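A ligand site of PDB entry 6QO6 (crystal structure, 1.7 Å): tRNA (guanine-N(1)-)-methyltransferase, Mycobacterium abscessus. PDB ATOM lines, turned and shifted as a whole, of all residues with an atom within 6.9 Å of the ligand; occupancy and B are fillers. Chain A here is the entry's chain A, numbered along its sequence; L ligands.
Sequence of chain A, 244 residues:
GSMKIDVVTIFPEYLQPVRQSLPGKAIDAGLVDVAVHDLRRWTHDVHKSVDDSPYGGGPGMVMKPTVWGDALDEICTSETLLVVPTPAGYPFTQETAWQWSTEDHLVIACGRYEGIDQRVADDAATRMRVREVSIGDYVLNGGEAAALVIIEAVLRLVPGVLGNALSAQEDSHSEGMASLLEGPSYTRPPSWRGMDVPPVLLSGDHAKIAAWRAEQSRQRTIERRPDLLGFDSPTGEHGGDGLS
The backbone carbonyl oxygen (O) of Gly 142 sits close to an oxygen (O1) of the ligand, at 3.5 Å.
Merely in contact with the ligand: Pro 85 (3.3 Å), Thr 86 (3.2 Å), Pro 87 (3.5 Å), Tyr 113 (3.3 Å), Ser 134 (3.5 Å), Gly 136 (3.2 Å), Leu 140 (3.1 Å), Asn 141 (3.9 Å) and Ala 146 (3.6 Å).
13 residues have an atom within 4 Å of the ligand: Pro 85, Thr 86, Pro 87, Tyr 113, Ser 134, Ile 135, Gly 136, Tyr 138, Leu 140, Asn 141, Gly 142, Gly 143 and Ala 146.
OH of Tyr 138 is in hydrogen-bond range of O of Ile 135 (3.3 Å).
OG1 of Thr 86 lies close to N of Ala 88, 3.0 Å away.
O of Val 133 sits at hydrogen-bond distance from N of Thr 86 (2.9 Å).
The backbone NH of Gly 143 sits at hydrogen-bond distance from the backbone carbonyl oxygen of Gly 111, 2.9 Å away.
O of Asn 141 lies within hydrogen-bond range of N of Tyr 113 (3.1 Å).
An oxygen (O1) of the ligand is in hydrogen-bond range of the backbone NH of Gly 143, at 3.5 Å.
N of Ile 135 sits at hydrogen-bond distance from N2 of the ligand (2.9 Å).
The backbone carbonyl oxygen (O) of Tyr 138 lies within hydrogen-bond range of a nitrogen (N1) of the ligand (2.7 Å).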
ATOM      1  N   VAL A  84      14.153  -0.061  16.400  1.00  0.00           N
ATOM      2  CA  VAL A  84      15.140   0.967  16.646  1.00  0.00           C
ATOM      3  C   VAL A  84      16.311   0.375  17.427  1.00  0.00           C
ATOM      4  O   VAL A  84      16.204   0.205  18.626  1.00  0.00           O
ATOM      5  CB  VAL A  84      14.562   2.145  17.461  1.00  0.00           C
ATOM      6  CG1 VAL A  84      15.601   3.259  17.614  1.00  0.00           C
ATOM      7  CG2 VAL A  84      13.284   2.666  16.838  1.00  0.00           C
ATOM      8  N   PRO A  85      17.402   0.019  16.731  1.00  0.00           N
ATOM      9  CA  PRO A  85      18.570  -0.489  17.453  1.00  0.00           C
ATOM     10  C   PRO A  85      19.191   0.559  18.381  1.00  0.00           C
ATOM     11  O   PRO A  85      19.463   1.689  17.955  1.00  0.00           O
ATOM     12  CB  PRO A  85      19.544  -0.873  16.329  1.00  0.00           C
ATOM     13  CG  PRO A  85      18.629  -1.146  15.149  1.00  0.00           C
ATOM     14  CD  PRO A  85      17.552  -0.118  15.274  1.00  0.00           C
ATOM     15  N   THR A  86      19.425   0.175  19.631  1.00  0.00           N
ATOM     16  CA  THR A  86      20.044   1.099  20.602  1.00  0.00           C
ATOM     17  C   THR A  86      20.653   0.288  21.714  1.00  0.00           C
ATOM     18  O   THR A  86      20.084  -0.726  22.141  1.00  0.00           O
ATOM     19  CB  THR A  86      19.026   2.131  21.174  1.00  0.00           C
ATOM     20  OG1 THR A  86      19.562   2.720  22.372  1.00  0.00           O
ATOM     21  CG2 THR A  86      17.701   1.497  21.497  1.00  0.00           C
ATOM     22  N   PRO A  87      21.828   0.711  22.205  1.00  0.00           N
ATOM     23  CA  PRO A  87      22.446  -0.017  23.308  1.00  0.00           C
ATOM     24  C   PRO A  87      21.574   0.010  24.562  1.00  0.00           C
ATOM     25  O   PRO A  87      21.782  -0.810  25.461  1.00  0.00           O
ATOM     26  CB  PRO A  87      23.781   0.733  23.530  1.00  0.00           C
ATOM     27  CG  PRO A  87      23.509   2.116  23.045  1.00  0.00           C
ATOM     28  CD  PRO A  87      22.546   1.960  21.878  1.00  0.00           C
ATOM     29  N   ALA A  88      20.619   0.932  24.605  1.00  0.00           N
ATOM     30  CA  ALA A  88      19.701   1.083  25.730  1.00  0.00           C
ATOM     31  C   ALA A  88      18.396   0.311  25.543  1.00  0.00           C
ATOM     32  O   ALA A  88      17.422   0.543  26.261  1.00  0.00           O
ATOM     33  CB  ALA A  88      19.402   2.581  25.960  1.00  0.00           C
ATOM     34  N   GLY A  89      18.362  -0.603  24.576  1.00  0.00           N
ATOM     35  CA  GLY A  89      17.136  -1.301  24.252  1.00  0.00           C
ATOM     36  C   GLY A  89      16.827  -2.529  25.104  1.00  0.00           C
ATOM     37  O   GLY A  89      17.657  -2.959  25.923  1.00  0.00           O
ATOM     38  N   GLY A 111      20.415   4.832  14.064  1.00  0.00           N
ATOM     39  CA  GLY A 111      20.910   6.107  14.550  1.00  0.00           C
ATOM     40  C   GLY A 111      22.269   5.981  15.204  1.00  0.00           C
ATOM     41  O   GLY A 111      22.752   4.892  15.476  1.00  0.00           O
ATOM     42  N   ARG A 112      22.902   7.114  15.464  1.00  0.00           N
ATOM     43  CA  ARG A 112      24.118   7.110  16.286  1.00  0.00           C
ATOM     44  C   ARG A 112      23.795   6.697  17.730  1.00  0.00           C
ATOM     45  O   ARG A 112      22.653   6.823  18.178  1.00  0.00           O
ATOM     46  CB  ARG A 112      24.754   8.493  16.242  1.00  0.00           C
ATOM     47  CG  ARG A 112      23.794   9.611  16.615  1.00  0.00           C
ATOM     48  CD  ARG A 112      24.467  10.943  16.285  1.00  0.00           C
ATOM     49  NE  ARG A 112      25.744  11.062  16.995  1.00  0.00           N
ATOM     50  CZ  ARG A 112      26.742  11.863  16.633  1.00  0.00           C
ATOM     51  NH1 ARG A 112      26.633  12.628  15.549  1.00  0.00           N
ATOM     52  NH2 ARG A 112      27.850  11.901  17.356  1.00  0.00           N
ATOM     53  N   TYR A 113      24.795   6.229  18.479  1.00  0.00           N
ATOM     54  CA  TYR A 113      24.511   5.612  19.785  1.00  0.00           C
ATOM     55  C   TYR A 113      24.002   6.615  20.818  1.00  0.00           C
ATOM     56  O   TYR A 113      23.271   6.226  21.746  1.00  0.00           O
ATOM     57  CB  TYR A 113      25.745   4.887  20.339  1.00  0.00           C
ATOM     58  CG  TYR A 113      26.792   5.753  20.995  1.00  0.00           C
ATOM     59  CD1 TYR A 113      27.714   6.459  20.237  1.00  0.00           C
ATOM     60  CD2 TYR A 113      26.874   5.841  22.376  1.00  0.00           C
ATOM     61  CE1 TYR A 113      28.683   7.251  20.838  1.00  0.00           C
ATOM     62  CE2 TYR A 113      27.835   6.626  22.990  1.00  0.00           C
ATOM     63  CZ  TYR A 113      28.739   7.325  22.211  1.00  0.00           C
ATOM     64  OH  TYR A 113      29.697   8.099  22.817  1.00  0.00           O
ATOM     65  N   GLU A 114      24.373   7.885  20.663  1.00  0.00           N
ATOM     66  CA  GLU A 114      23.889   8.963  21.538  1.00  0.00           C
ATOM     67  C   GLU A 114      22.385   9.109  21.435  1.00  0.00           C
ATOM     68  O   GLU A 114      21.726   9.604  22.358  1.00  0.00           O
ATOM     69  CB  GLU A 114      24.550  10.294  21.215  1.00  0.00           C
ATOM     70  CG  GLU A 114      26.054  10.339  21.450  1.00  0.00           C
ATOM     71  CD  GLU A 114      26.834  10.037  20.186  1.00  0.00           C
ATOM     72  OE1 GLU A 114      26.254   9.464  19.236  1.00  0.00           O
ATOM     73  OE2 GLU A 114      28.035  10.393  20.149  1.00  0.00           O
ATOM     74  N   VAL A 133      15.706  -2.003  20.694  1.00  0.00           N
ATOM     75  CA  VAL A 133      16.382  -3.247  21.046  1.00  0.00           C
ATOM     76  C   VAL A 133      17.893  -3.154  20.950  1.00  0.00           C
ATOM     77  O   VAL A 133      18.421  -2.456  20.079  1.00  0.00           O
ATOM     78  CB  VAL A 133      15.919  -4.450  20.147  1.00  0.00           C
ATOM     79  CG1 VAL A 133      14.453  -4.809  20.412  1.00  0.00           C
ATOM     80  CG2 VAL A 133      16.161  -4.169  18.644  1.00  0.00           C
ATOM     81  N   SER A 134      18.564  -3.865  21.843  1.00  0.00           N
ATOM     82  CA  SER A 134      20.030  -4.000  21.804  1.00  0.00           C
ATOM     83  C   SER A 134      20.397  -5.422  21.361  1.00  0.00           C
ATOM     84  O   SER A 134      19.695  -6.367  21.684  1.00  0.00           O
ATOM     85  CB  SER A 134      20.630  -3.699  23.171  1.00  0.00           C
ATOM     86  OG  SER A 134      20.266  -4.715  24.105  1.00  0.00           O
ATOM     87  N   ILE A 135      21.497  -5.554  20.629  1.00  0.00           N
ATOM     88  CA  ILE A 135      21.905  -6.903  20.219  1.00  0.00           C
ATOM     89  C   ILE A 135      22.996  -7.504  21.118  1.00  0.00           C
ATOM     90  O   ILE A 135      23.405  -8.657  20.932  1.00  0.00           O
ATOM     91  CB  ILE A 135      22.398  -6.931  18.746  1.00  0.00           C
ATOM     92  CG1 ILE A 135      23.553  -5.953  18.518  1.00  0.00           C
ATOM     93  CG2 ILE A 135      21.213  -6.659  17.763  1.00  0.00           C
ATOM     94  CD1 ILE A 135      24.390  -6.309  17.287  1.00  0.00           C
ATOM     95  N   GLY A 136      23.439  -6.763  22.139  1.00  0.00           N
ATOM     96  CA  GLY A 136      24.441  -7.292  23.040  1.00  0.00           C
ATOM     97  C   GLY A 136      24.949  -6.220  23.975  1.00  0.00           C
ATOM     98  O   GLY A 136      24.546  -5.069  23.892  1.00  0.00           O
ATOM     99  N   ASP A 137      25.850  -6.601  24.876  1.00  0.00           N
ATOM    100  CA  ASP A 137      26.369  -5.653  25.860  1.00  0.00           C
ATOM    101  C   ASP A 137      27.701  -5.065  25.422  1.00  0.00           C
ATOM    102  O   ASP A 137      28.740  -5.352  26.019  1.00  0.00           O
ATOM    103  CB  ASP A 137      26.533  -6.335  27.227  1.00  0.00           C
ATOM    104  CG  ASP A 137      25.210  -6.763  27.823  1.00  0.00           C
ATOM    105  OD1 ASP A 137      24.180  -6.152  27.479  1.00  0.00           O
ATOM    106  OD2 ASP A 137      25.191  -7.710  28.633  1.00  0.00           O
ATOM    107  N   TYR A 138      27.652  -4.251  24.384  1.00  0.00           N
ATOM    108  CA  TYR A 138      28.830  -3.541  23.900  1.00  0.00           C
ATOM    109  C   TYR A 138      28.301  -2.288  23.211  1.00  0.00           C
ATOM    110  O   TYR A 138      27.139  -2.226  22.811  1.00  0.00           O
ATOM    111  CB  TYR A 138      29.660  -4.402  22.951  1.00  0.00           C
ATOM    112  CG  TYR A 138      28.808  -5.326  22.104  1.00  0.00           C
ATOM    113  CD1 TYR A 138      28.106  -4.839  21.014  1.00  0.00           C
ATOM    114  CD2 TYR A 138      28.674  -6.670  22.436  1.00  0.00           C
ATOM    115  CE1 TYR A 138      27.291  -5.659  20.245  1.00  0.00           C
ATOM    116  CE2 TYR A 138      27.862  -7.525  21.664  1.00  0.00           C
ATOM    117  CZ  TYR A 138      27.174  -7.008  20.590  1.00  0.00           C
ATOM    118  OH  TYR A 138      26.356  -7.793  19.808  1.00  0.00           O
ATOM    119  N   VAL A 139      29.178  -1.302  23.085  1.00  0.00           N
ATOM    120  CA  VAL A 139      28.790  -0.049  22.448  1.00  0.00           C
ATOM    121  C   VAL A 139      29.307  -0.001  21.022  1.00  0.00           C
ATOM    122  O   VAL A 139      30.480  -0.287  20.772  1.00  0.00           O
ATOM    123  CB  VAL A 139      29.342   1.170  23.215  1.00  0.00           C
ATOM    124  CG1 VAL A 139      28.869   2.463  22.537  1.00  0.00           C
ATOM    125  CG2 VAL A 139      28.895   1.116  24.663  1.00  0.00           C
ATOM    126  N   LEU A 140      28.411   0.330  20.090  1.00  0.00           N
ATOM    127  CA  LEU A 140      28.786   0.571  18.701  1.00  0.00           C
ATOM    128  C   LEU A 140      28.619   2.047  18.414  1.00  0.00           C
ATOM    129  O   LEU A 140      27.862   2.719  19.112  1.00  0.00           O
ATOM    130  CB  LEU A 140      27.904  -0.234  17.754  1.00  0.00           C
ATOM    131  CG  LEU A 140      27.773  -1.706  18.092  1.00  0.00           C
ATOM    132  CD1 LEU A 140      26.762  -2.362  17.165  1.00  0.00           C
ATOM    133  CD2 LEU A 140      29.118  -2.353  17.952  1.00  0.00           C
ATOM    134  N   ASN A 141      29.284   2.552  17.378  1.00  0.00           N
ATOM    135  CA  ASN A 141      29.138   3.964  17.010  1.00  0.00           C
ATOM    136  C   ASN A 141      27.733   4.286  16.508  1.00  0.00           C
ATOM    137  O   ASN A 141      27.212   5.399  16.690  1.00  0.00           O
ATOM    138  CB  ASN A 141      30.140   4.341  15.937  1.00  0.00           C
ATOM    139  CG  ASN A 141      31.035   5.478  16.365  1.00  0.00           C
ATOM    140  OD1 ASN A 141      31.543   5.476  17.494  1.00  0.00           O
ATOM    141  ND2 ASN A 141      31.222   6.451  15.482  1.00  0.00           N
ATOM    142  N   GLY A 142      27.117   3.335  15.833  1.00  0.00           N
ATOM    143  CA  GLY A 142      25.797   3.547  15.269  1.00  0.00           C
ATOM    144  C   GLY A 142      25.048   2.234  15.110  1.00  0.00           C
ATOM    145  O   GLY A 142      25.618   1.184  15.343  1.00  0.00           O
ATOM    146  N   GLY A 143      23.777   2.313  14.738  1.00  0.00           N
ATOM    147  CA  GLY A 143      22.932   1.118  14.697  1.00  0.00           C
ATOM    148  C   GLY A 143      23.076   0.248  13.459  1.00  0.00           C
ATOM    149  O   GLY A 143      22.479  -0.834  13.394  1.00  0.00           O
ATOM    150  N   GLU A 144      23.861   0.686  12.478  1.00  0.00           N
ATOM    151  CA  GLU A 144      23.955  -0.030  11.199  1.00  0.00           C
ATOM    152  C   GLU A 144      24.403  -1.499  11.336  1.00  0.00           C
ATOM    153  O   GLU A 144      23.776  -2.399  10.770  1.00  0.00           O
ATOM    154  CB  GLU A 144      24.904   0.706  10.260  1.00  0.00           C
ATOM    155  CG  GLU A 144      24.273   1.938   9.589  1.00  0.00           C
ATOM    156  CD  GLU A 144      24.201   3.163  10.508  1.00  0.00           C
ATOM    157  OE1 GLU A 144      24.872   3.175  11.569  1.00  0.00           O
ATOM    158  OE2 GLU A 144      23.470   4.118  10.153  1.00  0.00           O
ATOM    159  N   ALA A 146      24.174  -3.383  13.909  1.00  0.00           N
ATOM    160  CA  ALA A 146      23.114  -4.094  14.621  1.00  0.00           C
ATOM    161  C   ALA A 146      21.948  -4.416  13.682  1.00  0.00           C
ATOM    162  O   ALA A 146      21.356  -5.500  13.773  1.00  0.00           O
ATOM    163  CB  ALA A 146      22.635  -3.277  15.814  1.00  0.00           C
ATOM    164  N   ALA A 147      21.630  -3.484  12.774  1.00  0.00           N
ATOM    165  CA  ALA A 147      20.604  -3.748  11.763  1.00  0.00           C
ATOM    166  C   ALA A 147      20.951  -4.943  10.879  1.00  0.00           C
ATOM    167  O   ALA A 147      20.063  -5.743  10.555  1.00  0.00           O
ATOM    168  CB  ALA A 147      20.381  -2.529  10.887  1.00  0.00           C
ATOM    169  N   ILE A 150      20.233  -8.078  12.954  1.00  0.00           N
ATOM    170  CA  ILE A 150      18.778  -8.282  13.051  1.00  0.00           C
ATOM    171  C   ILE A 150      18.195  -8.776  11.730  1.00  0.00           C
ATOM    172  O   ILE A 150      17.409  -9.734  11.703  1.00  0.00           O
ATOM    173  CB  ILE A 150      18.082  -6.985  13.488  1.00  0.00           C
ATOM    174  CG1 ILE A 150      18.496  -6.642  14.925  1.00  0.00           C
ATOM    175  CG2 ILE A 150      16.535  -7.108  13.333  1.00  0.00           C
ATOM    176  CD1 ILE A 150      18.152  -5.200  15.355  1.00  0.00           C
HETATM  177  N1  LIG L   1      25.017  -1.978  21.137  1.00  0.00           N
HETATM  178  N2  LIG L   1      23.236  -3.209  20.554  1.00  0.00           N
HETATM  179  C1  LIG L   1      24.387  -3.165  21.342  1.00  0.00           C
HETATM  180  C2  LIG L   1      23.152  -2.029  19.862  1.00  0.00           C
HETATM  181  C3  LIG L   1      24.278  -1.232  20.232  1.00  0.00           C
HETATM  182  C4  LIG L   1      24.472   0.061  19.672  1.00  0.00           C
HETATM  183  C5  LIG L   1      23.508   0.548  18.740  1.00  0.00           C
HETATM  184  C6  LIG L   1      22.362  -0.256  18.362  1.00  0.00           C
HETATM  185  C7  LIG L   1      22.175  -1.525  18.924  1.00  0.00           C
HETATM  186  O1  LIG L   1      23.662   1.827  18.165  1.00  0.00           O
HETATM  187  C8  LIG L   1      24.909   2.323  18.406  1.00  0.00           C
